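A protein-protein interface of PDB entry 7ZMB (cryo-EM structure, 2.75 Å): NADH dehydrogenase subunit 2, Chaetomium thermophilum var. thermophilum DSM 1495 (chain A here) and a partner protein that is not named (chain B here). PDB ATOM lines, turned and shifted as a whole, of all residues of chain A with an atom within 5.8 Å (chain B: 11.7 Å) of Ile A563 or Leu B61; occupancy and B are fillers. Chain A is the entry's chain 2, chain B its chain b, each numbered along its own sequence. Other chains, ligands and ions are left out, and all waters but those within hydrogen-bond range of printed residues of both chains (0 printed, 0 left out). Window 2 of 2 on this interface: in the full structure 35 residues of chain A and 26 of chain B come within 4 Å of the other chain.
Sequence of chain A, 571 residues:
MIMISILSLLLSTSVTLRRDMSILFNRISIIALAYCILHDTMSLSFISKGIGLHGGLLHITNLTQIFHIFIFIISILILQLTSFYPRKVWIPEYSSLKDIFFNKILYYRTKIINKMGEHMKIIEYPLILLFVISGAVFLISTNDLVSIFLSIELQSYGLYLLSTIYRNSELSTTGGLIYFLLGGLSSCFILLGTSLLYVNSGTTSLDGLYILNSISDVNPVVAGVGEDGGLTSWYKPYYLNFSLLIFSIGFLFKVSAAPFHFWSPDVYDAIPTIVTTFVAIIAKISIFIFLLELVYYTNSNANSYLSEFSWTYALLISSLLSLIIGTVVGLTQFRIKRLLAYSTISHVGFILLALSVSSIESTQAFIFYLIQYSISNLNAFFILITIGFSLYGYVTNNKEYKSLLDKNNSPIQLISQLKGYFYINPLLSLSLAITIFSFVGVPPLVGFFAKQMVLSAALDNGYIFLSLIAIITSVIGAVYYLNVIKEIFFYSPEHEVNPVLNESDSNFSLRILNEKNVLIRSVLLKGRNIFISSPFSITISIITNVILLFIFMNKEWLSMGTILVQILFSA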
ATOM      1  N   ILE A  47     -11.371  23.290  35.590  1.00  0.00           N
ATOM      2  CA  ILE A  47     -10.313  23.775  34.652  1.00  0.00           C
ATOM      3  C   ILE A  47     -10.361  25.301  34.647  1.00  0.00           C
ATOM      4  O   ILE A  47     -11.419  25.856  34.300  1.00  0.00           O
ATOM      5  CB  ILE A  47     -10.438  23.160  33.243  1.00  0.00           C
ATOM      6  CG1 ILE A  47     -10.290  21.637  33.270  1.00  0.00           C
ATOM      7  CG2 ILE A  47      -9.446  23.802  32.287  1.00  0.00           C
ATOM      8  CD1 ILE A  47      -8.936  21.162  33.736  1.00  0.00           C
ATOM      9  N   LEU A 558       4.591  13.294  32.063  1.00  0.00           N
ATOM     10  CA  LEU A 558       4.792  14.291  31.000  1.00  0.00           C
ATOM     11  C   LEU A 558       3.467  14.932  30.575  1.00  0.00           C
ATOM     12  O   LEU A 558       3.490  16.119  30.297  1.00  0.00           O
ATOM     13  CB  LEU A 558       5.624  13.644  29.881  1.00  0.00           C
ATOM     14  CG  LEU A 558       7.123  13.573  30.151  1.00  0.00           C
ATOM     15  CD1 LEU A 558       7.848  12.891  29.011  1.00  0.00           C
ATOM     16  CD2 LEU A 558       7.693  14.957  30.386  1.00  0.00           C
ATOM     17  N   SER A 559       2.379  14.162  30.498  1.00  0.00           N
ATOM     18  CA  SER A 559       1.027  14.657  30.119  1.00  0.00           C
ATOM     19  C   SER A 559       0.467  15.602  31.178  1.00  0.00           C
ATOM     20  O   SER A 559      -0.257  16.510  30.820  1.00  0.00           O
ATOM     21  CB  SER A 559       0.100  13.553  29.810  1.00  0.00           C
ATOM     22  OG  SER A 559       0.670  12.644  28.886  1.00  0.00           O
ATOM     23  N   MET A 560       0.815  15.365  32.437  1.00  0.00           N
ATOM     24  CA  MET A 560       0.384  16.247  33.527  1.00  0.00           C
ATOM     25  C   MET A 560       0.956  17.637  33.274  1.00  0.00           C
ATOM     26  O   MET A 560       0.232  18.612  33.504  1.00  0.00           O
ATOM     27  CB  MET A 560       0.924  15.744  34.855  1.00  0.00           C
ATOM     28  CG  MET A 560       0.504  16.589  36.044  1.00  0.00           C
ATOM     29  SD  MET A 560       1.639  16.462  37.447  1.00  0.00           S
ATOM     30  CE  MET A 560       2.982  17.510  36.895  1.00  0.00           C
ATOM     31  N   GLY A 561       2.176  17.711  32.749  1.00  0.00           N
ATOM     32  CA  GLY A 561       2.722  19.016  32.448  1.00  0.00           C
ATOM     33  C   GLY A 561       2.266  19.574  31.123  1.00  0.00           C
ATOM     34  O   GLY A 561       2.254  20.792  30.940  1.00  0.00           O
ATOM     35  N   THR A 562       1.899  18.708  30.180  1.00  0.00           N
ATOM     36  CA  THR A 562       1.318  19.186  28.933  1.00  0.00           C
ATOM     37  C   THR A 562      -0.002  19.900  29.194  1.00  0.00           C
ATOM     38  O   THR A 562      -0.275  20.955  28.616  1.00  0.00           O
ATOM     39  CB  THR A 562       1.105  18.015  27.974  1.00  0.00           C
ATOM     40  OG1 THR A 562       2.314  17.262  27.868  1.00  0.00           O
ATOM     41  CG2 THR A 562       0.724  18.519  26.593  1.00  0.00           C
ATOM     42  N   ILE A 563      -0.831  19.360  30.079  1.00  0.00           N
ATOM     43  CA  ILE A 563      -2.185  19.925  30.317  1.00  0.00           C
ATOM     44  C   ILE A 563      -2.083  21.218  31.126  1.00  0.00           C
ATOM     45  O   ILE A 563      -2.807  22.159  30.812  1.00  0.00           O
ATOM     46  CB  ILE A 563      -3.045  18.853  31.021  1.00  0.00           C
ATOM     47  CG1 ILE A 563      -3.318  17.672  30.090  1.00  0.00           C
ATOM     48  CG2 ILE A 563      -4.329  19.431  31.589  1.00  0.00           C
ATOM     49  CD1 ILE A 563      -3.888  16.462  30.774  1.00  0.00           C
ATOM     50  N   LEU A 564      -1.185  21.282  32.100  1.00  0.00           N
ATOM     51  CA  LEU A 564      -1.126  22.477  32.970  1.00  0.00           C
ATOM     52  C   LEU A 564      -0.726  23.659  32.097  1.00  0.00           C
ATOM     53  O   LEU A 564      -1.307  24.739  32.267  1.00  0.00           O
ATOM     54  CB  LEU A 564      -0.110  22.212  34.079  1.00  0.00           C
ATOM     55  CG  LEU A 564      -0.675  21.961  35.474  1.00  0.00           C
ATOM     56  CD1 LEU A 564      -1.919  21.094  35.415  1.00  0.00           C
ATOM     57  CD2 LEU A 564       0.377  21.324  36.368  1.00  0.00           C
ATOM     58  N   VAL A 565       0.229  23.445  31.193  1.00  0.00           N
ATOM     59  CA  VAL A 565       0.691  24.516  30.267  1.00  0.00           C
ATOM     60  C   VAL A 565      -0.432  24.926  29.321  1.00  0.00           C
ATOM     61  O   VAL A 565      -0.573  26.126  29.075  1.00  0.00           O
ATOM     62  CB  VAL A 565       1.983  24.111  29.544  1.00  0.00           C
ATOM     63  CG1 VAL A 565       2.468  25.200  28.609  1.00  0.00           C
ATOM     64  CG2 VAL A 565       3.060  23.778  30.561  1.00  0.00           C
ATOM     65  N   GLN A 566      -1.212  23.964  28.843  1.00  0.00           N
ATOM     66  CA  GLN A 566      -2.360  24.289  27.972  1.00  0.00           C
ATOM     67  C   GLN A 566      -3.347  25.167  28.741  1.00  0.00           C
ATOM     68  O   GLN A 566      -3.646  26.222  28.229  1.00  0.00           O
ATOM     69  CB  GLN A 566      -3.002  23.019  27.422  1.00  0.00           C
ATOM     70  CG  GLN A 566      -2.144  22.288  26.402  1.00  0.00           C
ATOM     71  CD  GLN A 566      -1.776  23.168  25.236  1.00  0.00           C
ATOM     72  OE1 GLN A 566      -2.635  23.753  24.585  1.00  0.00           O
ATOM     73  NE2 GLN A 566      -0.490  23.259  24.953  1.00  0.00           N
ATOM     74  N   ILE A 567      -3.661  24.856  29.995  1.00  0.00           N
ATOM     75  CA  ILE A 567      -4.562  25.750  30.774  1.00  0.00           C
ATOM     76  C   ILE A 567      -3.950  27.146  30.940  1.00  0.00           C
ATOM     77  O   ILE A 567      -4.676  28.111  30.693  1.00  0.00           O
ATOM     78  CB  ILE A 567      -4.950  25.100  32.112  1.00  0.00           C
ATOM     79  CG1 ILE A 567      -5.510  23.689  31.915  1.00  0.00           C
ATOM     80  CG2 ILE A 567      -5.910  25.983  32.893  1.00  0.00           C
ATOM     81  CD1 ILE A 567      -5.433  22.823  33.146  1.00  0.00           C
ATOM     82  N   LEU A 568      -2.664  27.254  31.263  1.00  0.00           N
ATOM     83  CA  LEU A 568      -2.004  28.562  31.515  1.00  0.00           C
ATOM     84  C   LEU A 568      -1.947  29.427  30.253  1.00  0.00           C
ATOM     85  O   LEU A 568      -1.998  30.655  30.395  1.00  0.00           O
ATOM     86  CB  LEU A 568      -0.614  28.312  32.101  1.00  0.00           C
ATOM     87  CG  LEU A 568       0.273  29.544  32.285  1.00  0.00           C
ATOM     88  CD1 LEU A 568      -0.104  30.313  33.540  1.00  0.00           C
ATOM     89  CD2 LEU A 568       1.741  29.155  32.327  1.00  0.00           C
ATOM     90  N   LEU B  50      -2.758   4.819  37.853  1.00  0.00           N
ATOM     91  CA  LEU B  50      -2.189   5.494  36.647  1.00  0.00           C
ATOM     92  C   LEU B  50      -3.043   5.245  35.414  1.00  0.00           C
ATOM     93  O   LEU B  50      -3.299   6.215  34.710  1.00  0.00           O
ATOM     94  CB  LEU B  50      -0.726   5.114  36.379  1.00  0.00           C
ATOM     95  CG  LEU B  50       0.316   5.951  37.105  1.00  0.00           C
ATOM     96  CD1 LEU B  50       1.663   5.808  36.424  1.00  0.00           C
ATOM     97  CD2 LEU B  50      -0.104   7.408  37.128  1.00  0.00           C
ATOM     98  N   SER B  52      -6.113   4.842  35.154  1.00  0.00           N
ATOM     99  CA  SER B  52      -7.318   5.658  35.219  1.00  0.00           C
ATOM    100  C   SER B  52      -7.028   7.114  34.885  1.00  0.00           C
ATOM    101  O   SER B  52      -7.737   7.723  34.078  1.00  0.00           O
ATOM    102  CB  SER B  52      -7.949   5.536  36.602  1.00  0.00           C
ATOM    103  OG  SER B  52      -7.364   6.451  37.509  1.00  0.00           O
ATOM    104  N   ILE B  53      -5.965   7.672  35.467  1.00  0.00           N
ATOM    105  CA  ILE B  53      -5.580   9.088  35.248  1.00  0.00           C
ATOM    106  C   ILE B  53      -5.101   9.253  33.811  1.00  0.00           C
ATOM    107  O   ILE B  53      -5.133  10.358  33.330  1.00  0.00           O
ATOM    108  CB  ILE B  53      -4.544   9.579  36.294  1.00  0.00           C
ATOM    109  CG1 ILE B  53      -3.100   9.240  35.921  1.00  0.00           C
ATOM    110  CG2 ILE B  53      -4.893   9.117  37.694  1.00  0.00           C
ATOM    111  CD1 ILE B  53      -2.265  10.449  35.602  1.00  0.00           C
ATOM    112  N   ASP B  54      -4.766   8.157  33.149  1.00  0.00           N
ATOM    113  CA  ASP B  54      -4.228   8.214  31.774  1.00  0.00           C
ATOM    114  C   ASP B  54      -5.449   8.352  30.892  1.00  0.00           C
ATOM    115  O   ASP B  54      -5.418   9.174  29.993  1.00  0.00           O
ATOM    116  CB  ASP B  54      -3.321   7.024  31.456  1.00  0.00           C
ATOM    117  CG  ASP B  54      -3.177   6.774  29.966  1.00  0.00           C
ATOM    118  OD1 ASP B  54      -2.539   7.599  29.289  1.00  0.00           O
ATOM    119  OD2 ASP B  54      -3.727   5.767  29.489  1.00  0.00           O
ATOM    120  N   GLU B  55      -6.513   7.630  31.228  1.00  0.00           N
ATOM    121  CA  GLU B  55      -7.768   7.801  30.500  1.00  0.00           C
ATOM    122  C   GLU B  55      -8.278   9.231  30.611  1.00  0.00           C
ATOM    123  O   GLU B  55      -8.824   9.780  29.649  1.00  0.00           O
ATOM    124  CB  GLU B  55      -8.827   6.827  31.012  1.00  0.00           C
ATOM    125  CG  GLU B  55      -8.403   5.375  31.049  1.00  0.00           C
ATOM    126  CD  GLU B  55      -8.981   4.627  32.239  1.00  0.00           C
ATOM    127  OE1 GLU B  55      -9.869   5.180  32.921  1.00  0.00           O
ATOM    128  OE2 GLU B  55      -8.549   3.482  32.492  1.00  0.00           O
ATOM    129  N   LYS B  56      -8.116   9.846  31.779  1.00  0.00           N
ATOM    130  CA  LYS B  56      -8.575  11.209  31.974  1.00  0.00           C
ATOM    131  C   LYS B  56      -7.685  12.225  31.273  1.00  0.00           C
ATOM    132  O   LYS B  56      -8.165  13.297  30.902  1.00  0.00           O
ATOM    133  CB  LYS B  56      -8.650  11.518  33.465  1.00  0.00           C
ATOM    134  CG  LYS B  56      -9.593  10.610  34.217  1.00  0.00           C
ATOM    135  CD  LYS B  56     -11.032  10.803  33.787  1.00  0.00           C
ATOM    136  CE  LYS B  56     -11.968  10.005  34.674  1.00  0.00           C
ATOM    137  NZ  LYS B  56     -11.811   8.542  34.456  1.00  0.00           N
ATOM    138  N   GLN B  57      -6.450  11.853  30.964  1.00  0.00           N
ATOM    139  CA  GLN B  57      -5.498  12.802  30.354  1.00  0.00           C
ATOM    140  C   GLN B  57      -5.643  12.728  28.844  1.00  0.00           C
ATOM    141  O   GLN B  57      -5.454  13.758  28.172  1.00  0.00           O
ATOM    142  CB  GLN B  57      -4.091  12.536  30.871  1.00  0.00           C
ATOM    143  CG  GLN B  57      -3.821  13.027  32.276  1.00  0.00           C
ATOM    144  CD  GLN B  57      -2.390  12.720  32.637  1.00  0.00           C
ATOM    145  OE1 GLN B  57      -1.755  11.853  32.040  1.00  0.00           O
ATOM    146  NE2 GLN B  57      -1.876  13.432  33.624  1.00  0.00           N
ATOM    147  N   THR B  58      -6.029  11.566  28.342  1.00  0.00           N
ATOM    148  CA  THR B  58      -6.276  11.459  26.913  1.00  0.00           C
ATOM    149  C   THR B  58      -7.452  12.328  26.503  1.00  0.00           C
ATOM    150  O   THR B  58      -7.392  13.026  25.484  1.00  0.00           O
ATOM    151  CB  THR B  58      -6.527  10.006  26.535  1.00  0.00           C
ATOM    152  OG1 THR B  58      -5.334   9.246  26.759  1.00  0.00           O
ATOM    153  CG2 THR B  58      -6.920   9.902  25.078  1.00  0.00           C
ATOM    154  N   LYS B  59      -8.519  12.312  27.299  1.00  0.00           N
ATOM    155  CA  LYS B  59      -9.690  13.125  27.008  1.00  0.00           C
ATOM    156  C   LYS B  59      -9.356  14.610  27.048  1.00  0.00           C
ATOM    157  O   LYS B  59      -9.679  15.350  26.114  1.00  0.00           O
ATOM    158  CB  LYS B  59     -10.801  12.790  28.000  1.00  0.00           C
ATOM    159  CG  LYS B  59     -11.928  13.787  28.037  1.00  0.00           C
ATOM    160  CD  LYS B  59     -13.019  13.345  29.000  1.00  0.00           C
ATOM    161  CE  LYS B  59     -14.197  12.725  28.265  1.00  0.00           C
ATOM    162  NZ  LYS B  59     -14.924  13.723  27.435  1.00  0.00           N
ATOM    163  N   MET B  60      -8.686  15.063  28.110  1.00  0.00           N
ATOM    164  CA  MET B  60      -8.423  16.490  28.252  1.00  0.00           C
ATOM    165  C   MET B  60      -7.575  17.027  27.105  1.00  0.00           C
ATOM    166  O   MET B  60      -7.827  18.125  26.602  1.00  0.00           O
ATOM    167  CB  MET B  60      -7.779  16.794  29.610  1.00  0.00           C
ATOM    168  CG  MET B  60      -8.692  16.548  30.806  1.00  0.00           C
ATOM    169  SD  MET B  60      -8.025  16.958  32.440  1.00  0.00           S
ATOM    170  CE  MET B  60      -6.861  15.644  32.771  1.00  0.00           C
ATOM    171  N   LEU B  61      -6.571  16.272  26.667  1.00  0.00           N
ATOM    172  CA  LEU B  61      -5.832  16.702  25.484  1.00  0.00           C
ATOM    173  C   LEU B  61      -6.634  16.494  24.206  1.00  0.00           C
ATOM    174  O   LEU B  61      -6.483  17.259  23.252  1.00  0.00           O
ATOM    175  CB  LEU B  61      -4.474  16.005  25.416  1.00  0.00           C
ATOM    176  CG  LEU B  61      -3.570  16.445  26.561  1.00  0.00           C
ATOM    177  CD1 LEU B  61      -2.260  15.671  26.600  1.00  0.00           C
ATOM    178  CD2 LEU B  61      -3.306  17.937  26.467  1.00  0.00           C
ATOM    179  N   GLU B  62      -7.499  15.479  24.166  1.00  0.00           N
ATOM    180  CA  GLU B  62      -8.375  15.321  23.010  1.00  0.00           C
ATOM    181  C   GLU B  62      -9.331  16.498  22.884  1.00  0.00           C
ATOM    182  O   GLU B  62      -9.561  17.002  21.781  1.00  0.00           O
ATOM    183  CB  GLU B  62      -9.151  14.011  23.101  1.00  0.00           C
ATOM    184  CG  GLU B  62      -9.980  13.707  21.872  1.00  0.00           C
ATOM    185  CD  GLU B  62      -9.132  13.508  20.628  1.00  0.00           C
ATOM    186  OE1 GLU B  62      -7.952  13.118  20.762  1.00  0.00           O
ATOM    187  OE2 GLU B  62      -9.645  13.745  19.516  1.00  0.00           O
ATOM    188  N   GLU B  63      -9.905  16.942  24.005  1.00  0.00           N
ATOM    189  CA  GLU B  63     -10.730  18.143  23.975  1.00  0.00           C
ATOM    190  C   GLU B  63      -9.913  19.365  23.589  1.00  0.00           C
ATOM    191  O   GLU B  63     -10.363  20.192  22.792  1.00  0.00           O
ATOM    192  CB  GLU B  63     -11.403  18.365  25.327  1.00  0.00           C
ATOM    193  CG  GLU B  63     -12.159  17.178  25.879  1.00  0.00           C
ATOM    194  CD  GLU B  63     -12.334  17.262  27.383  1.00  0.00           C
ATOM    195  OE1 GLU B  63     -11.610  18.053  28.022  1.00  0.00           O
ATOM    196  OE2 GLU B  63     -13.222  16.569  27.921  1.00  0.00           O
ATOM    197  N   ARG B  64      -8.711  19.495  24.145  1.00  0.00           N
ATOM    198  CA  ARG B  64      -7.877  20.653  23.848  1.00  0.00           C
ATOM    199  C   ARG B  64      -7.502  20.702  22.373  1.00  0.00           C
ATOM    200  O   ARG B  64      -7.600  21.754  21.738  1.00  0.00           O
ATOM    201  CB  ARG B  64      -6.625  20.630  24.728  1.00  0.00           C
ATOM    202  CG  ARG B  64      -5.668  21.766  24.481  1.00  0.00           C
ATOM    203  CD  ARG B  64      -6.166  23.045  25.108  1.00  0.00           C
ATOM    204  NE  ARG B  64      -5.462  24.229  24.620  1.00  0.00           N
ATOM    205  CZ  ARG B  64      -6.045  25.211  23.944  1.00  0.00           C
ATOM    206  NH1 ARG B  64      -7.331  25.145  23.657  1.00  0.00           N
ATOM    207  NH2 ARG B  64      -5.342  26.256  23.544  1.00  0.00           N
ATOM    208  N   LYS B  65      -7.083  19.569  21.801  1.00  0.00           N
ATOM    209  CA  LYS B  65      -6.706  19.573  20.390  1.00  0.00           C
ATOM    210  C   LYS B  65      -7.880  19.932  19.499  1.00  0.00           C
ATOM    211  O   LYS B  65      -7.704  20.635  18.499  1.00  0.00           O
ATOM    212  CB  LYS B  65      -6.092  18.232  19.974  1.00  0.00           C
ATOM    213  CG  LYS B  65      -4.774  17.927  20.684  1.00  0.00           C
ATOM    214  CD  LYS B  65      -4.128  16.637  20.220  1.00  0.00           C
ATOM    215  CE  LYS B  65      -4.868  15.389  20.666  1.00  0.00           C
ATOM    216  NZ  LYS B  65      -4.836  15.200  22.136  1.00  0.00           N
ATOM    217  N   GLN B  66      -9.083  19.483  19.848  1.00  0.00           N
ATOM    218  CA  GLN B  66     -10.270  19.967  19.154  1.00  0.00           C
ATOM    219  C   GLN B  66     -10.454  21.461  19.370  1.00  0.00           C
ATOM    220  O   GLN B  66     -10.685  22.212  18.418  1.00  0.00           O
ATOM    221  CB  GLN B  66     -11.495  19.192  19.618  1.00  0.00           C
ATOM    222  CG  GLN B  66     -11.467  17.731  19.228  1.00  0.00           C
ATOM    223  CD  GLN B  66     -10.654  17.479  17.973  1.00  0.00           C
ATOM    224  OE1 GLN B  66      -9.553  16.934  18.032  1.00  0.00           O
ATOM    225  NE2 GLN B  66     -11.203  17.865  16.825  1.00  0.00           N
ATOM    226  N   ALA B  67     -10.308  21.915  20.616  1.00  0.00           N
ATOM    227  CA  ALA B  67     -10.490  23.327  20.927  1.00  0.00           C
ATOM    228  C   ALA B  67      -9.459  24.211  20.236  1.00  0.00           C
ATOM    229  O   ALA B  67      -9.730  25.387  19.980  1.00  0.00           O
ATOM    230  CB  ALA B  67     -10.435  23.535  22.437  1.00  0.00           C
ATOM    231  N   ILE B  68      -8.270  23.685  19.949  1.00  0.00           N
ATOM    232  CA  ILE B  68      -7.280  24.470  19.219  1.00  0.00           C
ATOM    233  C   ILE B  68      -7.680  24.601  17.756  1.00  0.00           C
ATOM    234  O   ILE B  68      -7.671  25.700  17.192  1.00  0.00           O
ATOM    235  CB  ILE B  68      -5.877  23.860  19.373  1.00  0.00           C
ATOM    236  CG1 ILE B  68      -5.438  23.921  20.835  1.00  0.00           C
ATOM    237  CG2 ILE B  68      -4.893  24.599  18.504  1.00  0.00           C
ATOM    238  CD1 ILE B  68      -4.132  23.227  21.130  1.00  0.00           C
ATOM    239  N   LEU B  69      -8.065  23.487  17.128  1.00  0.00           N
ATOM    240  CA  LEU B  69      -8.506  23.527  15.738  1.00  0.00           C
ATOM    241  C   LEU B  69      -9.705  24.445  15.566  1.00  0.00           C
ATOM    242  O   LEU B  69      -9.757  25.239  14.623  1.00  0.00           O
ATOM    243  CB  LEU B  69      -8.868  22.125  15.255  1.00  0.00           C
ATOM    244  CG  LEU B  69      -7.799  21.058  15.072  1.00  0.00           C
ATOM    245  CD1 LEU B  69      -8.399  19.700  15.380  1.00  0.00           C
ATOM    246  CD2 LEU B  69      -7.250  21.099  13.665  1.00  0.00           C
ATOM    247  N   GLU B  70     -10.684  24.343  16.468  1.00  0.00           N
ATOM    248  CA  GLU B  70     -11.870  25.186  16.372  1.00  0.00           C
ATOM    249  C   GLU B  70     -11.523  26.655  16.558  1.00  0.00           C
ATOM    250  O   GLU B  70     -12.065  27.518  15.862  1.00  0.00           O
ATOM    251  CB  GLU B  70     -12.914  24.747  17.394  1.00  0.00           C
ATOM    252  CG  GLU B  70     -13.864  23.680  16.879  1.00  0.00           C
ATOM    253  CD  GLU B  70     -15.117  23.563  17.724  1.00  0.00           C
ATOM    254  OE1 GLU B  70     -15.352  24.455  18.566  1.00  0.00           O
ATOM    255  OE2 GLU B  70     -15.865  22.578  17.549  1.00  0.00           O
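Ile A563 touches three residues of chain B. Ser A559 touches one residue of chain B. No residue of chain B comes within 4 Å of Gly A561. Leu A564 touches none of the printed residues of chain B. No residue of chain B comes within 4 Å of Val A565. Gln A566 touches just these residues of chain B: Arg B64 and Ile B68. No residue of chain B comes within 4 Å of Ile A567. Of the printed residues of chain B, Met A560 touches Gln B57. Of the printed residues of chain A, Gln B57 touches Ser A559 (3.4 Å), Met A560 (3.5 Å) and Ile A563 (3.7 Å). Of the printed residues of chain A, Ile B68 touches Gln A566. Ile B53 touches none of the printed residues of chain A.
Ser A559 touches Gln B57 (CB to OE1, 3.4 Å). Met A560 touches Gln B57. CD1 of Ile A563 touches CG of Gln B57, at 3.7 Å. Met B60 touches Ile A563 (CE to CD1, 3.7 Å). Ile A563 touches Leu B61. Ile B68 touches Gln A566 (CD1 to OE1, 3.8 Å).
NZ of Lys B65 lies within hydrogen-bond range of O of Leu B61 (2.9 Å).
OE1 of Gln A566 sits at hydrogen-bond distance from NE of Arg B64 (2.9 Å).
Hydrophobic or aromatic side chains of chain B that line the printed part of chain A: Met B60, Leu B61 and Ile B68. Hydrophobic or aromatic side chains of chain A within 4 Å of the printed part of chain B: Met A560 and Ile A563.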
